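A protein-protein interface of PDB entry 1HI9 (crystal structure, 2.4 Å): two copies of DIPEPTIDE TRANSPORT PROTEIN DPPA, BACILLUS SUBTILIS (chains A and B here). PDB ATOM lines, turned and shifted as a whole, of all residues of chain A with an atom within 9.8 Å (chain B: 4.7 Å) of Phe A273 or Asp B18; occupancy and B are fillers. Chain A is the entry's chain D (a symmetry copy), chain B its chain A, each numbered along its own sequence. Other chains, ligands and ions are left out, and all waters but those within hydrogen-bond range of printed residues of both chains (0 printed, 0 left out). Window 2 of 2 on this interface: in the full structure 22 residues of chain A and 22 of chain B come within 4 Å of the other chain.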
ATOM      1  N   ALA A 224     -14.972  17.883  26.481  1.00  0.00           N
ATOM      2  CA  ALA A 224     -15.813  16.695  26.573  1.00  0.00           C
ATOM      3  C   ALA A 224     -16.036  16.002  25.230  1.00  0.00           C
ATOM      4  O   ALA A 224     -15.953  14.779  25.155  1.00  0.00           O
ATOM      5  CB  ALA A 224     -17.156  17.054  27.214  1.00  0.00           C
ATOM      6  N   ASN A 225     -16.335  16.772  24.180  1.00  0.00           N
ATOM      7  CA  ASN A 225     -16.563  16.192  22.853  1.00  0.00           C
ATOM      8  C   ASN A 225     -15.716  16.878  21.800  1.00  0.00           C
ATOM      9  O   ASN A 225     -15.101  17.914  22.072  1.00  0.00           O
ATOM     10  CB  ASN A 225     -18.044  16.267  22.460  1.00  0.00           C
ATOM     11  CG  ASN A 225     -18.563  17.691  22.377  1.00  0.00           C
ATOM     12  OD1 ASN A 225     -19.357  18.121  23.217  1.00  0.00           O
ATOM     13  ND2 ASN A 225     -18.115  18.436  21.359  1.00  0.00           N
ATOM     14  N   TYR A 226     -15.687  16.301  20.600  1.00  0.00           N
ATOM     15  CA  TYR A 226     -14.888  16.843  19.500  1.00  0.00           C
ATOM     16  C   TYR A 226     -15.424  18.178  18.968  1.00  0.00           C
ATOM     17  O   TYR A 226     -14.663  19.004  18.463  1.00  0.00           O
ATOM     18  CB  TYR A 226     -14.792  15.814  18.353  1.00  0.00           C
ATOM     19  CG  TYR A 226     -13.645  16.073  17.409  1.00  0.00           C
ATOM     20  CD1 TYR A 226     -12.336  15.707  17.743  1.00  0.00           C
ATOM     21  CD2 TYR A 226     -13.856  16.716  16.193  1.00  0.00           C
ATOM     22  CE1 TYR A 226     -11.272  15.983  16.882  1.00  0.00           C
ATOM     23  CE2 TYR A 226     -12.808  16.994  15.333  1.00  0.00           C
ATOM     24  CZ  TYR A 226     -11.522  16.633  15.678  1.00  0.00           C
ATOM     25  OH  TYR A 226     -10.490  16.958  14.823  1.00  0.00           O
ATOM     26  N   GLY A 227     -16.730  18.387  19.084  1.00  0.00           N
ATOM     27  CA  GLY A 227     -17.306  19.633  18.617  1.00  0.00           C
ATOM     28  C   GLY A 227     -16.737  20.827  19.372  1.00  0.00           C
ATOM     29  O   GLY A 227     -16.417  21.852  18.781  1.00  0.00           O
ATOM     30  N   GLN A 228     -16.597  20.702  20.683  1.00  0.00           N
ATOM     31  CA  GLN A 228     -16.056  21.806  21.470  1.00  0.00           C
ATOM     32  C   GLN A 228     -14.603  22.049  21.094  1.00  0.00           C
ATOM     33  O   GLN A 228     -14.140  23.182  21.102  1.00  0.00           O
ATOM     34  CB  GLN A 228     -16.193  21.507  22.962  1.00  0.00           C
ATOM     35  CG  GLN A 228     -17.629  21.168  23.343  1.00  0.00           C
ATOM     36  CD  GLN A 228     -17.723  20.389  24.631  1.00  0.00           C
ATOM     37  OE1 GLN A 228     -16.966  19.441  24.859  1.00  0.00           O
ATOM     38  NE2 GLN A 228     -18.668  20.762  25.473  1.00  0.00           N
ATOM     39  N   TRP A 231     -14.518  24.097  17.801  1.00  0.00           N
ATOM     40  CA  TRP A 231     -14.807  25.502  18.042  1.00  0.00           C
ATOM     41  C   TRP A 231     -13.549  26.222  18.539  1.00  0.00           C
ATOM     42  O   TRP A 231     -13.150  27.257  17.982  1.00  0.00           O
ATOM     43  CB  TRP A 231     -15.932  25.658  19.069  1.00  0.00           C
ATOM     44  CG  TRP A 231     -17.313  25.875  18.490  1.00  0.00           C
ATOM     45  CD1 TRP A 231     -18.351  24.985  18.483  1.00  0.00           C
ATOM     46  CD2 TRP A 231     -17.816  27.077  17.897  1.00  0.00           C
ATOM     47  NE1 TRP A 231     -19.468  25.557  17.940  1.00  0.00           N
ATOM     48  CE2 TRP A 231     -19.175  26.841  17.565  1.00  0.00           C
ATOM     49  CE3 TRP A 231     -17.259  28.333  17.616  1.00  0.00           C
ATOM     50  CZ2 TRP A 231     -19.985  27.819  16.960  1.00  0.00           C
ATOM     51  CZ3 TRP A 231     -18.072  29.305  17.014  1.00  0.00           C
ATOM     52  CH2 TRP A 231     -19.418  29.037  16.697  1.00  0.00           C
ATOM     53  N   ALA A 268     -15.982  27.151  22.914  1.00  0.00           N
ATOM     54  CA  ALA A 268     -16.475  25.808  23.171  1.00  0.00           C
ATOM     55  C   ALA A 268     -17.888  25.830  23.726  1.00  0.00           C
ATOM     56  O   ALA A 268     -18.649  24.913  23.471  1.00  0.00           O
ATOM     57  CB  ALA A 268     -15.546  25.095  24.130  1.00  0.00           C
ATOM     58  N   MET A 269     -18.224  26.880  24.470  1.00  0.00           N
ATOM     59  CA  MET A 269     -19.550  27.043  25.056  1.00  0.00           C
ATOM     60  C   MET A 269     -20.663  27.085  24.005  1.00  0.00           C
ATOM     61  O   MET A 269     -21.804  26.770  24.305  1.00  0.00           O
ATOM     62  CB  MET A 269     -19.603  28.331  25.882  1.00  0.00           C
ATOM     63  CG  MET A 269     -19.556  28.123  27.373  1.00  0.00           C
ATOM     64  SD  MET A 269     -21.088  27.394  27.989  1.00  0.00           S
ATOM     65  CE  MET A 269     -22.019  28.893  28.398  1.00  0.00           C
ATOM     66  N   ARG A 270     -20.328  27.470  22.781  1.00  0.00           N
ATOM     67  CA  ARG A 270     -21.322  27.565  21.717  1.00  0.00           C
ATOM     68  C   ARG A 270     -21.699  26.219  21.112  1.00  0.00           C
ATOM     69  O   ARG A 270     -22.693  26.119  20.388  1.00  0.00           O
ATOM     70  CB  ARG A 270     -20.819  28.494  20.602  1.00  0.00           C
ATOM     71  CG  ARG A 270     -20.391  29.871  21.094  1.00  0.00           C
ATOM     72  CD  ARG A 270     -21.547  30.575  21.788  1.00  0.00           C
ATOM     73  NE  ARG A 270     -22.209  31.542  20.910  1.00  0.00           N
ATOM     74  CZ  ARG A 270     -21.653  32.681  20.501  1.00  0.00           C
ATOM     75  NH1 ARG A 270     -20.423  32.994  20.895  1.00  0.00           N
ATOM     76  NH2 ARG A 270     -22.321  33.510  19.706  1.00  0.00           N
ATOM     77  N   THR A 271     -20.913  25.187  21.410  1.00  0.00           N
ATOM     78  CA  THR A 271     -21.156  23.851  20.860  1.00  0.00           C
ATOM     79  C   THR A 271     -22.567  23.319  21.101  1.00  0.00           C
ATOM     80  O   THR A 271     -23.079  23.335  22.219  1.00  0.00           O
ATOM     81  CB  THR A 271     -20.146  22.833  21.406  1.00  0.00           C
ATOM     82  OG1 THR A 271     -18.817  23.351  21.243  1.00  0.00           O
ATOM     83  CG2 THR A 271     -20.269  21.508  20.646  1.00  0.00           C
ATOM     84  N   SER A 272     -23.182  22.848  20.022  1.00  0.00           N
ATOM     85  CA  SER A 272     -24.529  22.309  20.065  1.00  0.00           C
ATOM     86  C   SER A 272     -24.492  20.781  20.055  1.00  0.00           C
ATOM     87  O   SER A 272     -23.436  20.176  19.844  1.00  0.00           O
ATOM     88  CB  SER A 272     -25.327  22.807  18.858  1.00  0.00           C
ATOM     89  OG  SER A 272     -24.799  22.274  17.654  1.00  0.00           O
ATOM     90  N   PHE A 273     -25.656  20.169  20.270  1.00  0.00           N
ATOM     91  CA  PHE A 273     -25.793  18.715  20.294  1.00  0.00           C
ATOM     92  C   PHE A 273     -24.927  18.109  21.395  1.00  0.00           C
ATOM     93  O   PHE A 273     -24.072  17.257  21.144  1.00  0.00           O
ATOM     94  CB  PHE A 273     -25.413  18.123  18.930  1.00  0.00           C
ATOM     95  CG  PHE A 273     -25.840  16.689  18.741  1.00  0.00           C
ATOM     96  CD1 PHE A 273     -27.192  16.336  18.780  1.00  0.00           C
ATOM     97  CD2 PHE A 273     -24.892  15.695  18.496  1.00  0.00           C
ATOM     98  CE1 PHE A 273     -27.598  15.016  18.574  1.00  0.00           C
ATOM     99  CE2 PHE A 273     -25.281  14.369  18.288  1.00  0.00           C
ATOM    100  CZ  PHE A 273     -26.640  14.025  18.327  1.00  0.00           C
ATOM    101  N   CYS A 274     -25.147  18.571  22.621  1.00  0.00           N
ATOM    102  CA  CYS A 274     -24.411  18.069  23.774  1.00  0.00           C
ATOM    103  C   CYS A 274     -25.052  18.596  25.059  1.00  0.00           C
ATOM    104  O   CYS A 274     -24.480  18.483  26.133  1.00  0.00           O
ATOM    105  CB  CYS A 274     -22.935  18.498  23.703  1.00  0.00           C
ATOM    106  SG  CYS A 274     -22.595  20.288  23.886  1.00  0.00           S
ATOM    107  N   GLU B  10     -28.299   9.914  12.922  1.00  0.00           N
ATOM    108  CA  GLU B  10     -27.213  10.865  12.718  1.00  0.00           C
ATOM    109  C   GLU B  10     -26.391  10.630  11.461  1.00  0.00           C
ATOM    110  O   GLU B  10     -25.894  11.575  10.851  1.00  0.00           O
ATOM    111  CB  GLU B  10     -26.284  10.892  13.930  1.00  0.00           C
ATOM    112  CG  GLU B  10     -26.905  11.486  15.184  1.00  0.00           C
ATOM    113  CD  GLU B  10     -27.781  10.501  15.938  1.00  0.00           C
ATOM    114  OE1 GLU B  10     -27.931   9.357  15.466  1.00  0.00           O
ATOM    115  OE2 GLU B  10     -28.313  10.871  17.007  1.00  0.00           O
ATOM    116  N   ASP B  17     -27.152  18.378  11.006  1.00  0.00           N
ATOM    117  CA  ASP B  17     -27.210  18.662  12.440  1.00  0.00           C
ATOM    118  C   ASP B  17     -28.423  18.068  13.145  1.00  0.00           C
ATOM    119  O   ASP B  17     -29.247  17.411  12.522  1.00  0.00           O
ATOM    120  CB  ASP B  17     -27.159  20.175  12.654  1.00  0.00           C
ATOM    121  CG  ASP B  17     -28.240  20.908  11.878  1.00  0.00           C
ATOM    122  OD1 ASP B  17     -27.892  21.747  11.016  1.00  0.00           O
ATOM    123  OD2 ASP B  17     -29.438  20.647  12.136  1.00  0.00           O
ATOM    124  N   ASP B  18     -28.544  18.327  14.438  1.00  0.00           N
ATOM    125  CA  ASP B  18     -29.632  17.753  15.208  1.00  0.00           C
ATOM    126  C   ASP B  18     -31.031  18.303  14.940  1.00  0.00           C
ATOM    127  O   ASP B  18     -32.004  17.747  15.436  1.00  0.00           O
ATOM    128  CB  ASP B  18     -29.310  17.820  16.706  1.00  0.00           C
ATOM    129  CG  ASP B  18     -29.439  19.215  17.279  1.00  0.00           C
ATOM    130  OD1 ASP B  18     -29.461  20.193  16.517  1.00  0.00           O
ATOM    131  OD2 ASP B  18     -29.510  19.342  18.521  1.00  0.00           O
ATOM    132  N   THR B  19     -31.149  19.374  14.162  1.00  0.00           N
ATOM    133  CA  THR B  19     -32.471  19.892  13.858  1.00  0.00           C
ATOM    134  C   THR B  19     -33.197  18.852  12.992  1.00  0.00           C
ATOM    135  O   THR B  19     -34.411  18.902  12.850  1.00  0.00           O
ATOM    136  CB  THR B  19     -32.425  21.226  13.081  1.00  0.00           C
ATOM    137  OG1 THR B  19     -31.901  21.005  11.765  1.00  0.00           O
ATOM    138  CG2 THR B  19     -31.537  22.242  13.810  1.00  0.00           C
ATOM    139  N   PHE B  20     -32.443  17.916  12.414  1.00  0.00           N
ATOM    140  CA  PHE B  20     -33.010  16.862  11.589  1.00  0.00           C
ATOM    141  C   PHE B  20     -33.225  15.543  12.356  1.00  0.00           C
ATOM    142  O   PHE B  20     -33.898  14.647  11.856  1.00  0.00           O
ATOM    143  CB  PHE B  20     -32.105  16.558  10.381  1.00  0.00           C
ATOM    144  CG  PHE B  20     -32.056  17.644   9.343  1.00  0.00           C
ATOM    145  CD1 PHE B  20     -31.302  18.789   9.554  1.00  0.00           C
ATOM    146  CD2 PHE B  20     -32.760  17.516   8.145  1.00  0.00           C
ATOM    147  CE1 PHE B  20     -31.243  19.791   8.600  1.00  0.00           C
ATOM    148  CE2 PHE B  20     -32.706  18.519   7.179  1.00  0.00           C
ATOM    149  CZ  PHE B  20     -31.945  19.656   7.412  1.00  0.00           C
ATOM    150  N   VAL B  21     -32.661  15.405  13.553  1.00  0.00           N
ATOM    151  CA  VAL B  21     -32.807  14.149  14.296  1.00  0.00           C
ATOM    152  C   VAL B  21     -33.494  14.278  15.648  1.00  0.00           C
ATOM    153  O   VAL B  21     -33.823  13.282  16.274  1.00  0.00           O
ATOM    154  CB  VAL B  21     -31.429  13.472  14.531  1.00  0.00           C
ATOM    155  CG1 VAL B  21     -30.641  13.450  13.235  1.00  0.00           C
ATOM    156  CG2 VAL B  21     -30.659  14.207  15.615  1.00  0.00           C
ATOM    157  N   ASP B  22     -33.703  15.501  16.104  1.00  0.00           N
ATOM    158  CA  ASP B  22     -34.346  15.725  17.393  1.00  0.00           C
ATOM    159  C   ASP B  22     -35.846  15.877  17.129  1.00  0.00           C
ATOM    160  O   ASP B  22     -36.254  16.845  16.494  1.00  0.00           O
ATOM    161  CB  ASP B  22     -33.778  17.001  18.013  1.00  0.00           C
ATOM    162  CG  ASP B  22     -34.207  17.202  19.446  1.00  0.00           C
ATOM    163  OD1 ASP B  22     -35.420  17.074  19.734  1.00  0.00           O
ATOM    164  OD2 ASP B  22     -33.323  17.506  20.280  1.00  0.00           O
ATOM    165  N   LYS B  25     -37.414  19.262  17.084  1.00  0.00           N
ATOM    166  CA  LYS B  25     -36.898  20.352  16.254  1.00  0.00           C
ATOM    167  C   LYS B  25     -37.466  20.475  14.844  1.00  0.00           C
ATOM    168  O   LYS B  25     -37.957  19.505  14.255  1.00  0.00           O
ATOM    169  CB  LYS B  25     -35.376  20.286  16.175  1.00  0.00           C
ATOM    170  CG  LYS B  25     -34.656  20.546  17.480  1.00  0.00           C
ATOM    171  CD  LYS B  25     -33.166  20.363  17.262  1.00  0.00           C
ATOM    172  CE  LYS B  25     -32.393  20.302  18.557  1.00  0.00           C
ATOM    173  NZ  LYS B  25     -32.393  21.602  19.234  1.00  0.00           N
ATOM    174  N   MET B 113     -22.029  14.718  14.365  1.00  0.00           N
ATOM    175  CA  MET B 113     -22.864  14.295  15.489  1.00  0.00           C
ATOM    176  C   MET B 113     -22.314  13.099  16.253  1.00  0.00           C
ATOM    177  O   MET B 113     -23.063  12.229  16.679  1.00  0.00           O
ATOM    178  CB  MET B 113     -24.279  13.998  14.997  1.00  0.00           C
ATOM    179  CG  MET B 113     -24.942  15.213  14.359  1.00  0.00           C
ATOM    180  SD  MET B 113     -26.650  14.903  13.781  1.00  0.00           S
ATOM    181  CE  MET B 113     -27.461  15.219  15.253  1.00  0.00           C
ATOM    182  N   HIS B 115     -21.059  10.654  19.052  1.00  0.00           N
ATOM    183  CA  HIS B 115     -21.461  10.383  20.432  1.00  0.00           C
ATOM    184  C   HIS B 115     -21.662   8.885  20.575  1.00  0.00           C
ATOM    185  O   HIS B 115     -21.556   8.161  19.592  1.00  0.00           O
ATOM    186  CB  HIS B 115     -22.760  11.108  20.788  1.00  0.00           C
ATOM    187  CG  HIS B 115     -23.954  10.590  20.051  1.00  0.00           C
ATOM    188  ND1 HIS B 115     -24.194  10.885  18.725  1.00  0.00           N
ATOM    189  CD2 HIS B 115     -24.948   9.758  20.435  1.00  0.00           C
ATOM    190  CE1 HIS B 115     -25.286  10.260  18.328  1.00  0.00           C
ATOM    191  NE2 HIS B 115     -25.764   9.570  19.347  1.00  0.00           N
ATOM    192  N   PHE B 119     -25.079  11.785  25.544  1.00  0.00           N
ATOM    193  CA  PHE B 119     -24.073  12.841  25.458  1.00  0.00           C
ATOM    194  C   PHE B 119     -23.011  12.680  26.533  1.00  0.00           C
ATOM    195  O   PHE B 119     -21.856  13.062  26.342  1.00  0.00           O
ATOM    196  CB  PHE B 119     -24.736  14.218  25.604  1.00  0.00           C
ATOM    197  CG  PHE B 119     -25.641  14.584  24.452  1.00  0.00           C
ATOM    198  CD1 PHE B 119     -26.902  15.145  24.687  1.00  0.00           C
ATOM    199  CD2 PHE B 119     -25.230  14.385  23.135  1.00  0.00           C
ATOM    200  CE1 PHE B 119     -27.745  15.492  23.629  1.00  0.00           C
ATOM    201  CE2 PHE B 119     -26.061  14.727  22.065  1.00  0.00           C
ATOM    202  CZ  PHE B 119     -27.321  15.285  22.315  1.00  0.00           C
ATOM    203  N   ARG B 179     -18.482  18.560  13.507  1.00  0.00           N
ATOM    204  CA  ARG B 179     -19.461  17.768  14.232  1.00  0.00           C
ATOM    205  C   ARG B 179     -20.897  18.145  13.826  1.00  0.00           C
ATOM    206  O   ARG B 179     -21.836  17.409  14.107  1.00  0.00           O
ATOM    207  CB  ARG B 179     -19.264  17.935  15.743  1.00  0.00           C
ATOM    208  CG  ARG B 179     -20.036  16.935  16.601  1.00  0.00           C
ATOM    209  CD  ARG B 179     -19.366  16.805  17.948  1.00  0.00           C
ATOM    210  NE  ARG B 179     -20.067  15.917  18.855  1.00  0.00           N
ATOM    211  CZ  ARG B 179     -21.117  16.274  19.584  1.00  0.00           C
ATOM    212  NH1 ARG B 179     -21.589  17.511  19.498  1.00  0.00           N
ATOM    213  NH2 ARG B 179     -21.676  15.400  20.422  1.00  0.00           N
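Among the printed residues, merely in contact across the chains: Gly A227 with Arg B179 (3.3 Å), Phe A273 with Asp B18 (3.3 Å), Phe A273 with Met B113 (3.3 Å), Phe A273 with Phe B119 (3.3 Å), Phe A273 with His B115 (3.7 Å), Cys A274 with Phe B119 (3.8 Å), Phe A273 with Glu B10 (3.8 Å) and Asn A225 with Arg B179 (3.98 Å).
Tyr A226 touches none of the printed residues of chain B. Of the printed residues of chain B, Ser A272 touches Arg B179. Phe A273 touches just these residues of chain B: Glu B10 (3.8 Å), Asp B18 (3.3 Å), Met B113 (3.3 Å), His B115 (3.7 Å), Phe B119 (3.3 Å) and Arg B179 (3.0 Å). Printed residues of chain A within 4 Å of Glu B10: Phe A273. No residue of chain A comes within 4 Å of Asp B17. Of chain A, only Phe A273 (3.3 Å) comes within 4 Å of Asp B18. No residue of chain A comes within 4 Å of Thr B19. No residue of chain A comes within 4 Å of Val B21. No residue of chain A comes within 4 Å of Asp B22. Lys B25 touches none of the printed residues of chain A. Printed residues of chain A within 4 Å of Met B113: Phe A273 (3.3 Å). Of the printed residues of chain A, Phe B119 touches Phe A273 and Cys A274. The nearest residue of chain A that does not touch Asp B18 is Ser A272 (5.2 Å). The nearest printed residue of chain A that does not touch Phe B119 is Ala A224 (6.2 Å).
Printed residues of chain A that touch a printed residue of chain B: Asn A225, Gly A227, Ser A272, Phe A273 and Cys A274. Hydrophobic or aromatic side chains of chain A that line the printed part of chain B: Phe A273. Printed residues of chain B that touch a printed residue of chain A: Glu B10, Asp B18, Met B113, His B115, Phe B119 and Arg B179. Among the printed residues, 10 pairs touch across the chains.
The side-chain carboxylate of Asp B18 lies within salt-bridge range of the side-chain amino group of Lys B25 (3.7 Å). The backbone carbonyl oxygen (O) of Met B113 sits at hydrogen-bond distance from a ring nitrogen (ND1) of His B115 (2.7 Å). N of Met B113 sits at hydrogen-bond distance from O of Arg B179. The side-chain amide nitrogen (ND2) of Asn A225 sits close to the backbone NH (N) of Gly A227. The side-chain amide nitrogen (ND2) of Asn A225 lies close to the backbone NH (N) of Gln A228 (2.8 Å). SG of Cys A274 sits at hydrogen-bond distance from O of Thr A271, 3.5 Å away.
No position is printed for both chains. Of the 10 pairs that touch across the chains among the printed residues, none has its exchanged pair printed and touching as well.
O of Ser A272 sits at hydrogen-bond distance from NH1 of Arg B179. The guanidinium group (NH1) of Arg B179 sits at hydrogen-bond distance from the backbone carbonyl oxygen (O) of Phe A273 (3.0 Å).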
